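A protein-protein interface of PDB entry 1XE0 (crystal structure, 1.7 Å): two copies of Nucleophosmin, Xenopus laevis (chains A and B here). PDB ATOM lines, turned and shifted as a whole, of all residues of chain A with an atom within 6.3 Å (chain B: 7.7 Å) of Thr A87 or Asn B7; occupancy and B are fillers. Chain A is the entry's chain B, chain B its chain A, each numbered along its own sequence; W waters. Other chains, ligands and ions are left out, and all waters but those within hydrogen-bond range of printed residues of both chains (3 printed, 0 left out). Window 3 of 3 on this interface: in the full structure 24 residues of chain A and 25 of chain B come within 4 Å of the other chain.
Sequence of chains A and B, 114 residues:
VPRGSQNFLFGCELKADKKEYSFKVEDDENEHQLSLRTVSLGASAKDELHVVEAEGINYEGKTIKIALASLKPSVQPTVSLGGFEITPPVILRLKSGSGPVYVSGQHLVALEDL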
ATOM      1  N   PHE A  23       7.019 -14.795  22.252  1.00  0.00           N
ATOM      2  CA  PHE A  23       7.995 -15.002  21.160  1.00  0.00           C
ATOM      3  C   PHE A  23       7.638 -16.299  20.509  1.00  0.00           C
ATOM      4  O   PHE A  23       7.724 -17.344  21.130  1.00  0.00           O
ATOM      5  CB  PHE A  23       9.474 -14.919  21.647  1.00  0.00           C
ATOM      6  CG  PHE A  23      10.448 -15.068  20.582  1.00  0.00           C
ATOM      7  CD1 PHE A  23      10.753 -13.975  19.716  1.00  0.00           C
ATOM      8  CD2 PHE A  23      11.008 -16.313  20.328  1.00  0.00           C
ATOM      9  CE1 PHE A  23      11.684 -14.147  18.651  1.00  0.00           C
ATOM     10  CE2 PHE A  23      11.965 -16.516  19.253  1.00  0.00           C
ATOM     11  CZ  PHE A  23      12.281 -15.437  18.400  1.00  0.00           C
ATOM     12  N   GLU A  31      16.181 -23.040  12.150  1.00  0.00           N
ATOM     13  CA  GLU A  31      16.405 -22.978  13.603  1.00  0.00           C
ATOM     14  C   GLU A  31      16.365 -21.500  13.965  1.00  0.00           C
ATOM     15  O   GLU A  31      17.009 -20.640  13.302  1.00  0.00           O
ATOM     16  CB  GLU A  31      17.704 -23.679  14.048  1.00  0.00           C
ATOM     17  CG  GLU A  31      17.843 -25.171  13.634  1.00  0.00           C
ATOM     18  CD  GLU A  31      16.496 -25.974  13.741  1.00  0.00           C
ATOM     19  OE1 GLU A  31      15.729 -25.689  14.718  1.00  0.00           O
ATOM     20  OE2 GLU A  31      16.170 -26.896  12.908  1.00  0.00           O
ATOM     21  N   HIS A  32      15.510 -21.195  14.946  1.00  0.00           N
ATOM     22  CA  HIS A  32      15.433 -19.852  15.485  1.00  0.00           C
ATOM     23  C   HIS A  32      15.805 -19.959  16.920  1.00  0.00           C
ATOM     24  O   HIS A  32      15.516 -20.980  17.574  1.00  0.00           O
ATOM     25  CB  HIS A  32      14.021 -19.329  15.388  1.00  0.00           C
ATOM     26  CG  HIS A  32      13.561 -19.176  13.987  1.00  0.00           C
ATOM     27  ND1 HIS A  32      13.308 -17.934  13.437  1.00  0.00           N
ATOM     28  CD2 HIS A  32      13.368 -20.089  12.999  1.00  0.00           C
ATOM     29  CE1 HIS A  32      12.919 -18.106  12.182  1.00  0.00           C
ATOM     30  NE2 HIS A  32      12.996 -19.390  11.874  1.00  0.00           N
ATOM     31  N   GLN A  33      16.471 -18.929  17.394  1.00  0.00           N
ATOM     32  CA  GLN A  33      16.697 -18.775  18.804  1.00  0.00           C
ATOM     33  C   GLN A  33      16.511 -17.328  19.177  1.00  0.00           C
ATOM     34  O   GLN A  33      16.833 -16.430  18.432  1.00  0.00           O
ATOM     35  CB  GLN A  33      18.158 -19.157  19.167  1.00  0.00           C
ATOM     36  CG  GLN A  33      18.583 -20.524  18.873  1.00  0.00           C
ATOM     37  CD  GLN A  33      18.044 -21.480  19.902  1.00  0.00           C
ATOM     38  OE1 GLN A  33      17.689 -21.082  21.037  1.00  0.00           O
ATOM     39  NE2 GLN A  33      17.891 -22.730  19.512  1.00  0.00           N
ATOM     40  N   LEU A  34      16.013 -17.107  20.374  1.00  0.00           N
ATOM     41  CA  LEU A  34      15.953 -15.772  20.969  1.00  0.00           C
ATOM     42  C   LEU A  34      17.133 -15.739  21.876  1.00  0.00           C
ATOM     43  O   LEU A  34      17.188 -16.497  22.795  1.00  0.00           O
ATOM     44  CB  LEU A  34      14.651 -15.598  21.712  1.00  0.00           C
ATOM     45  CG  LEU A  34      14.463 -14.317  22.481  1.00  0.00           C
ATOM     46  CD1 LEU A  34      14.503 -13.076  21.573  1.00  0.00           C
ATOM     47  CD2 LEU A  34      13.270 -14.276  23.377  1.00  0.00           C
ATOM     48  N   GLY A  56       8.737 -21.588  28.986  1.00  0.00           N
ATOM     49  CA  GLY A  56       9.081 -22.342  27.774  1.00  0.00           C
ATOM     50  C   GLY A  56       9.264 -23.851  28.083  1.00  0.00           C
ATOM     51  O   GLY A  56       9.092 -24.276  29.210  1.00  0.00           O
ATOM     52  N   ILE A  57       9.761 -24.592  27.098  1.00  0.00           N
ATOM     53  CA  ILE A  57       9.816 -26.013  27.202  1.00  0.00           C
ATOM     54  C   ILE A  57      11.073 -26.518  27.885  1.00  0.00           C
ATOM     55  O   ILE A  57      12.147 -26.139  27.501  1.00  0.00           O
ATOM     56  CB  ILE A  57       9.724 -26.442  25.661  1.00  0.00           C
ATOM     57  CG1 ILE A  57       8.335 -26.040  25.164  1.00  0.00           C
ATOM     58  CG2 ILE A  57       9.936 -27.744  25.474  1.00  0.00           C
ATOM     59  CD1 ILE A  57       7.243 -26.591  25.996  1.00  0.00           C
ATOM     60  N   GLU A  85      20.360 -18.041  25.045  1.00  0.00           N
ATOM     61  CA  GLU A  85      19.506 -18.486  23.934  1.00  0.00           C
ATOM     62  C   GLU A  85      18.391 -19.338  24.399  1.00  0.00           C
ATOM     63  O   GLU A  85      18.612 -20.252  25.148  1.00  0.00           O
ATOM     64  CB  GLU A  85      20.364 -19.316  22.947  1.00  0.00           C
ATOM     65  CG  GLU A  85      21.487 -18.479  22.381  1.00  0.00           C
ATOM     66  CD  GLU A  85      22.252 -19.008  21.174  1.00  0.00           C
ATOM     67  OE1 GLU A  85      23.274 -18.336  20.855  1.00  0.00           O
ATOM     68  OE2 GLU A  85      21.806 -19.931  20.473  1.00  0.00           O
ATOM     69  N   ILE A  86      17.203 -19.032  23.924  1.00  0.00           N
ATOM     70  CA  ILE A  86      16.044 -19.822  24.175  1.00  0.00           C
ATOM     71  C   ILE A  86      15.347 -20.174  22.845  1.00  0.00           C
ATOM     72  O   ILE A  86      15.214 -19.332  21.946  1.00  0.00           O
ATOM     73  CB  ILE A  86      15.051 -19.069  25.066  1.00  0.00           C
ATOM     74  CG1 ILE A  86      15.739 -18.631  26.331  1.00  0.00           C
ATOM     75  CG2 ILE A  86      13.842 -20.005  25.299  1.00  0.00           C
ATOM     76  CD1 ILE A  86      14.913 -17.704  27.333  1.00  0.00           C
ATOM     77  N   THR A  87      14.988 -21.431  22.708  1.00  0.00           N
ATOM     78  CA  THR A  87      14.205 -21.923  21.543  1.00  0.00           C
ATOM     79  C   THR A  87      12.738 -21.516  21.649  1.00  0.00           C
ATOM     80  O   THR A  87      12.153 -21.729  22.688  1.00  0.00           O
ATOM     81  CB  THR A  87      14.284 -23.449  21.492  1.00  0.00           C
ATOM     82  OG1 THR A  87      15.679 -23.840  21.428  1.00  0.00           O
ATOM     83  CG2 THR A  87      13.648 -23.936  20.223  1.00  0.00           C
ATOM     84  N   PRO A  88      12.131 -20.907  20.603  1.00  0.00           N
ATOM     85  CA  PRO A  88      10.723 -20.594  20.640  1.00  0.00           C
ATOM     86  C   PRO A  88       9.889 -21.863  20.740  1.00  0.00           C
ATOM     87  O   PRO A  88      10.321 -22.922  20.300  1.00  0.00           O
ATOM     88  CB  PRO A  88      10.466 -19.856  19.321  1.00  0.00           C
ATOM     89  CG  PRO A  88      11.518 -20.424  18.410  1.00  0.00           C
ATOM     90  CD  PRO A  88      12.764 -20.565  19.320  1.00  0.00           C
ATOM     91  N   PRO A  89       8.687 -21.755  21.254  1.00  0.00           N
ATOM     92  CA  PRO A  89       8.100 -20.522  21.773  1.00  0.00           C
ATOM     93  C   PRO A  89       8.456 -20.229  23.207  1.00  0.00           C
ATOM     94  O   PRO A  89       8.659 -21.169  23.935  1.00  0.00           O
ATOM     95  CB  PRO A  89       6.604 -20.780  21.671  1.00  0.00           C
ATOM     96  CG  PRO A  89       6.463 -22.190  21.736  1.00  0.00           C
ATOM     97  CD  PRO A  89       7.723 -22.885  21.213  1.00  0.00           C
ATOM     98  N   VAL A  90       8.538 -18.951  23.549  1.00  0.00           N
ATOM     99  CA  VAL A  90       8.773 -18.564  24.951  1.00  0.00           C
ATOM    100  C   VAL A  90       8.005 -17.294  25.265  1.00  0.00           C
ATOM    101  O   VAL A  90       7.869 -16.458  24.433  1.00  0.00           O
ATOM    102  CB  VAL A  90      10.272 -18.448  25.259  1.00  0.00           C
ATOM    103  CG1 VAL A  90      10.902 -17.423  24.310  1.00  0.00           C
ATOM    104  CG2 VAL A  90      10.558 -18.072  26.665  1.00  0.00           C
ATOM    105  N   ARG B   3      24.815 -22.815  20.790  1.00  0.00           N
ATOM    106  CA  ARG B   3      25.005 -23.234  19.355  1.00  0.00           C
ATOM    107  C   ARG B   3      25.323 -24.709  19.130  1.00  0.00           C
ATOM    108  O   ARG B   3      26.229 -25.251  19.803  1.00  0.00           O
ATOM    109  N   GLY B   4      24.526 -25.345  18.226  1.00  0.00           N
ATOM    110  CA  GLY B   4      24.825 -26.584  17.514  1.00  0.00           C
ATOM    111  C   GLY B   4      23.811 -27.730  17.609  1.00  0.00           C
ATOM    112  O   GLY B   4      23.118 -28.031  16.585  1.00  0.00           O
ATOM    113  N   SER B   5      23.905 -28.428  18.772  1.00  0.00           N
ATOM    114  CA  SER B   5      22.997 -29.357  19.474  1.00  0.00           C
ATOM    115  C   SER B   5      21.668 -28.742  20.046  1.00  0.00           C
ATOM    116  O   SER B   5      21.309 -27.681  19.649  1.00  0.00           O
ATOM    117  CB  SER B   5      23.812 -29.812  20.653  1.00  0.00           C
ATOM    118  OG  SER B   5      24.048 -28.708  21.534  1.00  0.00           O
ATOM    119  N   GLN B   6      20.888 -29.380  20.926  1.00  0.00           N
ATOM    120  CA  GLN B   6      19.554 -28.833  21.230  1.00  0.00           C
ATOM    121  C   GLN B   6      19.589 -28.108  22.571  1.00  0.00           C
ATOM    122  O   GLN B   6      20.410 -28.436  23.376  1.00  0.00           O
ATOM    123  CB  GLN B   6      18.566 -29.963  21.324  1.00  0.00           C
ATOM    124  CG  GLN B   6      18.369 -30.632  19.958  1.00  0.00           C
ATOM    125  CD  GLN B   6      17.382 -31.641  20.032  1.00  0.00           C
ATOM    126  OE1 GLN B   6      16.191 -31.359  20.261  1.00  0.00           O
ATOM    127  NE2 GLN B   6      17.836 -32.888  19.946  1.00  0.00           N
ATOM    128  N   ASN B   7      18.741 -27.115  22.780  1.00  0.00           N
ATOM    129  CA  ASN B   7      18.762 -26.353  24.072  1.00  0.00           C
ATOM    130  C   ASN B   7      17.376 -26.202  24.601  1.00  0.00           C
ATOM    131  O   ASN B   7      16.469 -25.835  23.905  1.00  0.00           O
ATOM    132  CB  ASN B   7      19.467 -24.930  24.178  1.00  0.00           C
ATOM    133  CG  ASN B   7      18.947 -23.965  23.209  1.00  0.00           C
ATOM    134  OD1 ASN B   7      18.555 -22.778  23.538  1.00  0.00           O
ATOM    135  ND2 ASN B   7      19.001 -24.400  21.953  1.00  0.00           N
ATOM    136  N   PHE B   8      17.210 -26.582  25.844  1.00  0.00           N
ATOM    137  CA  PHE B   8      15.934 -26.505  26.510  1.00  0.00           C
ATOM    138  C   PHE B   8      16.111 -25.640  27.710  1.00  0.00           C
ATOM    139  O   PHE B   8      17.187 -25.595  28.260  1.00  0.00           O
ATOM    140  CB  PHE B   8      15.582 -27.926  26.920  1.00  0.00           C
ATOM    141  CG  PHE B   8      15.390 -28.834  25.722  1.00  0.00           C
ATOM    142  CD1 PHE B   8      16.388 -29.649  25.266  1.00  0.00           C
ATOM    143  CD2 PHE B   8      14.142 -28.903  25.136  1.00  0.00           C
ATOM    144  CE1 PHE B   8      16.193 -30.476  24.199  1.00  0.00           C
ATOM    145  CE2 PHE B   8      13.982 -29.708  24.033  1.00  0.00           C
ATOM    146  CZ  PHE B   8      15.026 -30.519  23.630  1.00  0.00           C
ATOM    147  N   LEU B   9      15.033 -25.080  28.211  1.00  0.00           N
ATOM    148  CA  LEU B   9      15.135 -24.275  29.429  1.00  0.00           C
ATOM    149  C   LEU B   9      15.335 -25.104  30.661  1.00  0.00           C
ATOM    150  O   LEU B   9      14.748 -26.124  30.817  1.00  0.00           O
ATOM    151  CB  LEU B   9      13.862 -23.485  29.661  1.00  0.00           C
ATOM    152  CG  LEU B   9      13.385 -22.405  28.791  1.00  0.00           C
ATOM    153  CD1 LEU B   9      12.196 -21.737  29.331  1.00  0.00           C
ATOM    154  CD2 LEU B   9      14.438 -21.369  28.649  1.00  0.00           C
ATOM    155  N   PHE B  10      16.104 -24.590  31.626  1.00  0.00           N
ATOM    156  CA  PHE B  10      16.277 -25.217  32.906  1.00  0.00           C
ATOM    157  C   PHE B  10      16.062 -24.176  34.020  1.00  0.00           C
ATOM    158  O   PHE B  10      16.504 -23.008  33.888  1.00  0.00           O
ATOM    159  CB  PHE B  10      17.670 -25.735  33.064  1.00  0.00           C
ATOM    160  CG  PHE B  10      17.941 -26.158  34.493  1.00  0.00           C
ATOM    161  CD1 PHE B  10      17.354 -27.349  34.955  1.00  0.00           C
ATOM    162  CD2 PHE B  10      18.489 -25.285  35.399  1.00  0.00           C
ATOM    163  CE1 PHE B  10      17.473 -27.782  36.289  1.00  0.00           C
ATOM    164  CE2 PHE B  10      18.621 -25.699  36.751  1.00  0.00           C
ATOM    165  CZ  PHE B  10      18.118 -26.956  37.197  1.00  0.00           C
ATOM    166  N   GLY B 105      18.935 -21.594  33.452  1.00  0.00           N
ATOM    167  CA  GLY B 105      19.908 -21.936  32.455  1.00  0.00           C
ATOM    168  C   GLY B 105      19.339 -22.774  31.359  1.00  0.00           C
ATOM    169  O   GLY B 105      18.163 -22.740  31.068  1.00  0.00           O
ATOM    170  N   GLN B 106      20.224 -23.526  30.717  1.00  0.00           N
ATOM    171  CA  GLN B 106      19.929 -24.277  29.530  1.00  0.00           C
ATOM    172  C   GLN B 106      20.325 -25.697  29.794  1.00  0.00           C
ATOM    173  O   GLN B 106      21.356 -25.998  30.415  1.00  0.00           O
ATOM    174  CB  GLN B 106      20.727 -23.780  28.359  1.00  0.00           C
ATOM    175  CG  GLN B 106      20.493 -22.327  27.938  1.00  0.00           C
ATOM    176  CD  GLN B 106      21.566 -21.826  27.073  1.00  0.00           C
ATOM    177  OE1 GLN B 106      21.336 -21.062  26.141  1.00  0.00           O
ATOM    178  NE2 GLN B 106      22.766 -22.361  27.295  1.00  0.00           N
ATOM    179  N   HIS B 107      19.512 -26.620  29.339  1.00  0.00           N
ATOM    180  CA  HIS B 107      19.896 -27.996  29.327  1.00  0.00           C
ATOM    181  C   HIS B 107      20.254 -28.242  27.882  1.00  0.00           C
ATOM    182  O   HIS B 107      19.383 -28.156  27.002  1.00  0.00           O
ATOM    183  CB  HIS B 107      18.717 -28.816  29.789  1.00  0.00           C
ATOM    184  CG  HIS B 107      18.930 -30.295  29.902  1.00  0.00           C
ATOM    185  ND1 HIS B 107      19.804 -31.041  29.155  1.00  0.00           N
ATOM    186  CD2 HIS B 107      18.161 -31.199  30.571  1.00  0.00           C
ATOM    187  CE1 HIS B 107      19.687 -32.314  29.496  1.00  0.00           C
ATOM    188  NE2 HIS B 107      18.644 -32.436  30.295  1.00  0.00           N
ATOM    189  N   LEU B 108      21.504 -28.576  27.613  1.00  0.00           N
ATOM    190  CA  LEU B 108      22.016 -28.778  26.272  1.00  0.00           C
ATOM    191  C   LEU B 108      22.143 -30.288  25.971  1.00  0.00           C
ATOM    192  O   LEU B 108      22.591 -31.037  26.835  1.00  0.00           O
ATOM    193  CB  LEU B 108      23.389 -28.171  26.157  1.00  0.00           C
ATOM    194  CG  LEU B 108      23.393 -26.682  26.457  1.00  0.00           C
ATOM    195  CD1 LEU B 108      24.797 -26.177  26.291  1.00  0.00           C
ATOM    196  CD2 LEU B 108      22.457 -25.994  25.521  1.00  0.00           C
ATOM    197  N   VAL B 109      21.702 -30.719  24.792  1.00  0.00           N
ATOM    198  CA  VAL B 109      21.661 -32.146  24.434  1.00  0.00           C
ATOM    199  C   VAL B 109      22.376 -32.322  23.086  1.00  0.00           C
ATOM    200  O   VAL B 109      21.942 -31.676  22.121  1.00  0.00           O
ATOM    201  CB  VAL B 109      20.172 -32.635  24.231  1.00  0.00           C
ATOM    202  CG1 VAL B 109      20.189 -34.157  24.063  1.00  0.00           C
ATOM    203  CG2 VAL B 109      19.375 -32.267  25.412  1.00  0.00           C
ATOM    204  N   ALA B 110      23.456 -33.114  22.986  1.00  0.00           N
ATOM    205  CA  ALA B 110      24.039 -33.412  21.646  1.00  0.00           C
ATOM    206  C   ALA B 110      24.163 -34.916  21.450  1.00  0.00           C
ATOM    207  O   ALA B 110      24.339 -35.665  22.370  1.00  0.00           O
ATOM    208  CB  ALA B 110      25.381 -32.707  21.396  1.00  0.00           C
HETATM  209  O   HOH W   1      17.386 -22.586  26.469  1.00  0.00           O
HETATM  210  O   HOH W   2      15.192 -23.298  24.952  1.00  0.00           O
HETATM  211  O   HOH W   3      16.789 -26.516  20.689  1.00  0.00           O
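Among the printed residues, merely in contact across the chains: Gly A56 with Leu B9, Ile A86 with Leu B9, Ile A57 with Phe B8 and Ile A86 with Asn B7.
No position is printed for both chains.
Of the 9 pairs that touch across the chains among the printed residues, none has its exchanged pair printed and touching as well.
Water W3 bridges N of Asn B7 and OG1 of Thr A87.
Water W2 bridges the backbone NH (N) of Thr A87 (2.9 Å) and the backbone carbonyl oxygen (O) of Asn B7 (3.0 Å).
Water W1 bridges O of Glu A85 (2.9 Å) and OD1 of Asn B7 (3.2 Å).
The side-chain amide nitrogen of Gln A33 lies within hydrogen-bond range of the side-chain hydroxyl of Thr A87 (3.1 Å).
The backbone NH (N) of Ile A86 sits at hydrogen-bond distance from the backbone carbonyl oxygen (O) of Leu A34 (2.8 Å).
The backbone carbonyl oxygen (O) of Phe B8 is in hydrogen-bond range of the backbone NH (N) of His B107.
The side-chain amide oxygen (OE1) of Gln A33 lies close to the backbone carbonyl oxygen (O) of Ile A86 (3.2 Å).
OE1 of Gln A33 sits close to OD1 of Asn B7, 3.1 Å away.
OE1 of Gln B106 lies close to O of Glu A85 (3.0 Å).
O of Asn B7 is in hydrogen-bond range of OG1 of Thr A87 (3.3 Å).
The backbone carbonyl oxygen (O) of Ile A57 lies within hydrogen-bond range of the backbone NH (N) of Leu B9 (3.2 Å).
The side-chain amide oxygen of Asn B7 lies close to the backbone carbonyl oxygen of Glu A85 (3.0 Å).
Printed residues of chain B within 4 Å of Gln A33: Asn B7.
Leu A34 touches none of the printed residues of chain B.
Printed residues of chain B within 4 Å of Glu A85: Asn B7 and Gln B106.
Of the printed residues of chain B, Ile A86 touches Asn B7 (3.9 Å) and Leu B9 (3.7 Å).
Thr A87 touches just one residue of chain B: Asn B7.
Asn B7 touches four residues of chain A.
Of the printed residues of chain A, Leu B9 touches Gly A56 (3.5 Å), Ile A57 (3.2 Å) and Ile A86 (3.7 Å).
The nearest residue of chain B that does not touch Thr A87 is Phe B8 (5.4 Å).
The nearest residue of chain A that does not touch Asn B7 is Ile A57 (5.6 Å).
The nearest printed residue of chain B that does not touch Ile A86 is Gln B106 (5.1 Å).
Printed residues of chain B that touch a printed residue of chain A: Asn B7, Phe B8, Leu B9 and Gln B106.
Hydrophobic or aromatic side chains of chain B within 4 Å of the printed part of chain A: Phe B8 and Leu B9.
Among the printed residues, no Asp or Glu carboxylate lies within 4 Å of a Lys or Arg side-chain nitrogen of the other chain.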
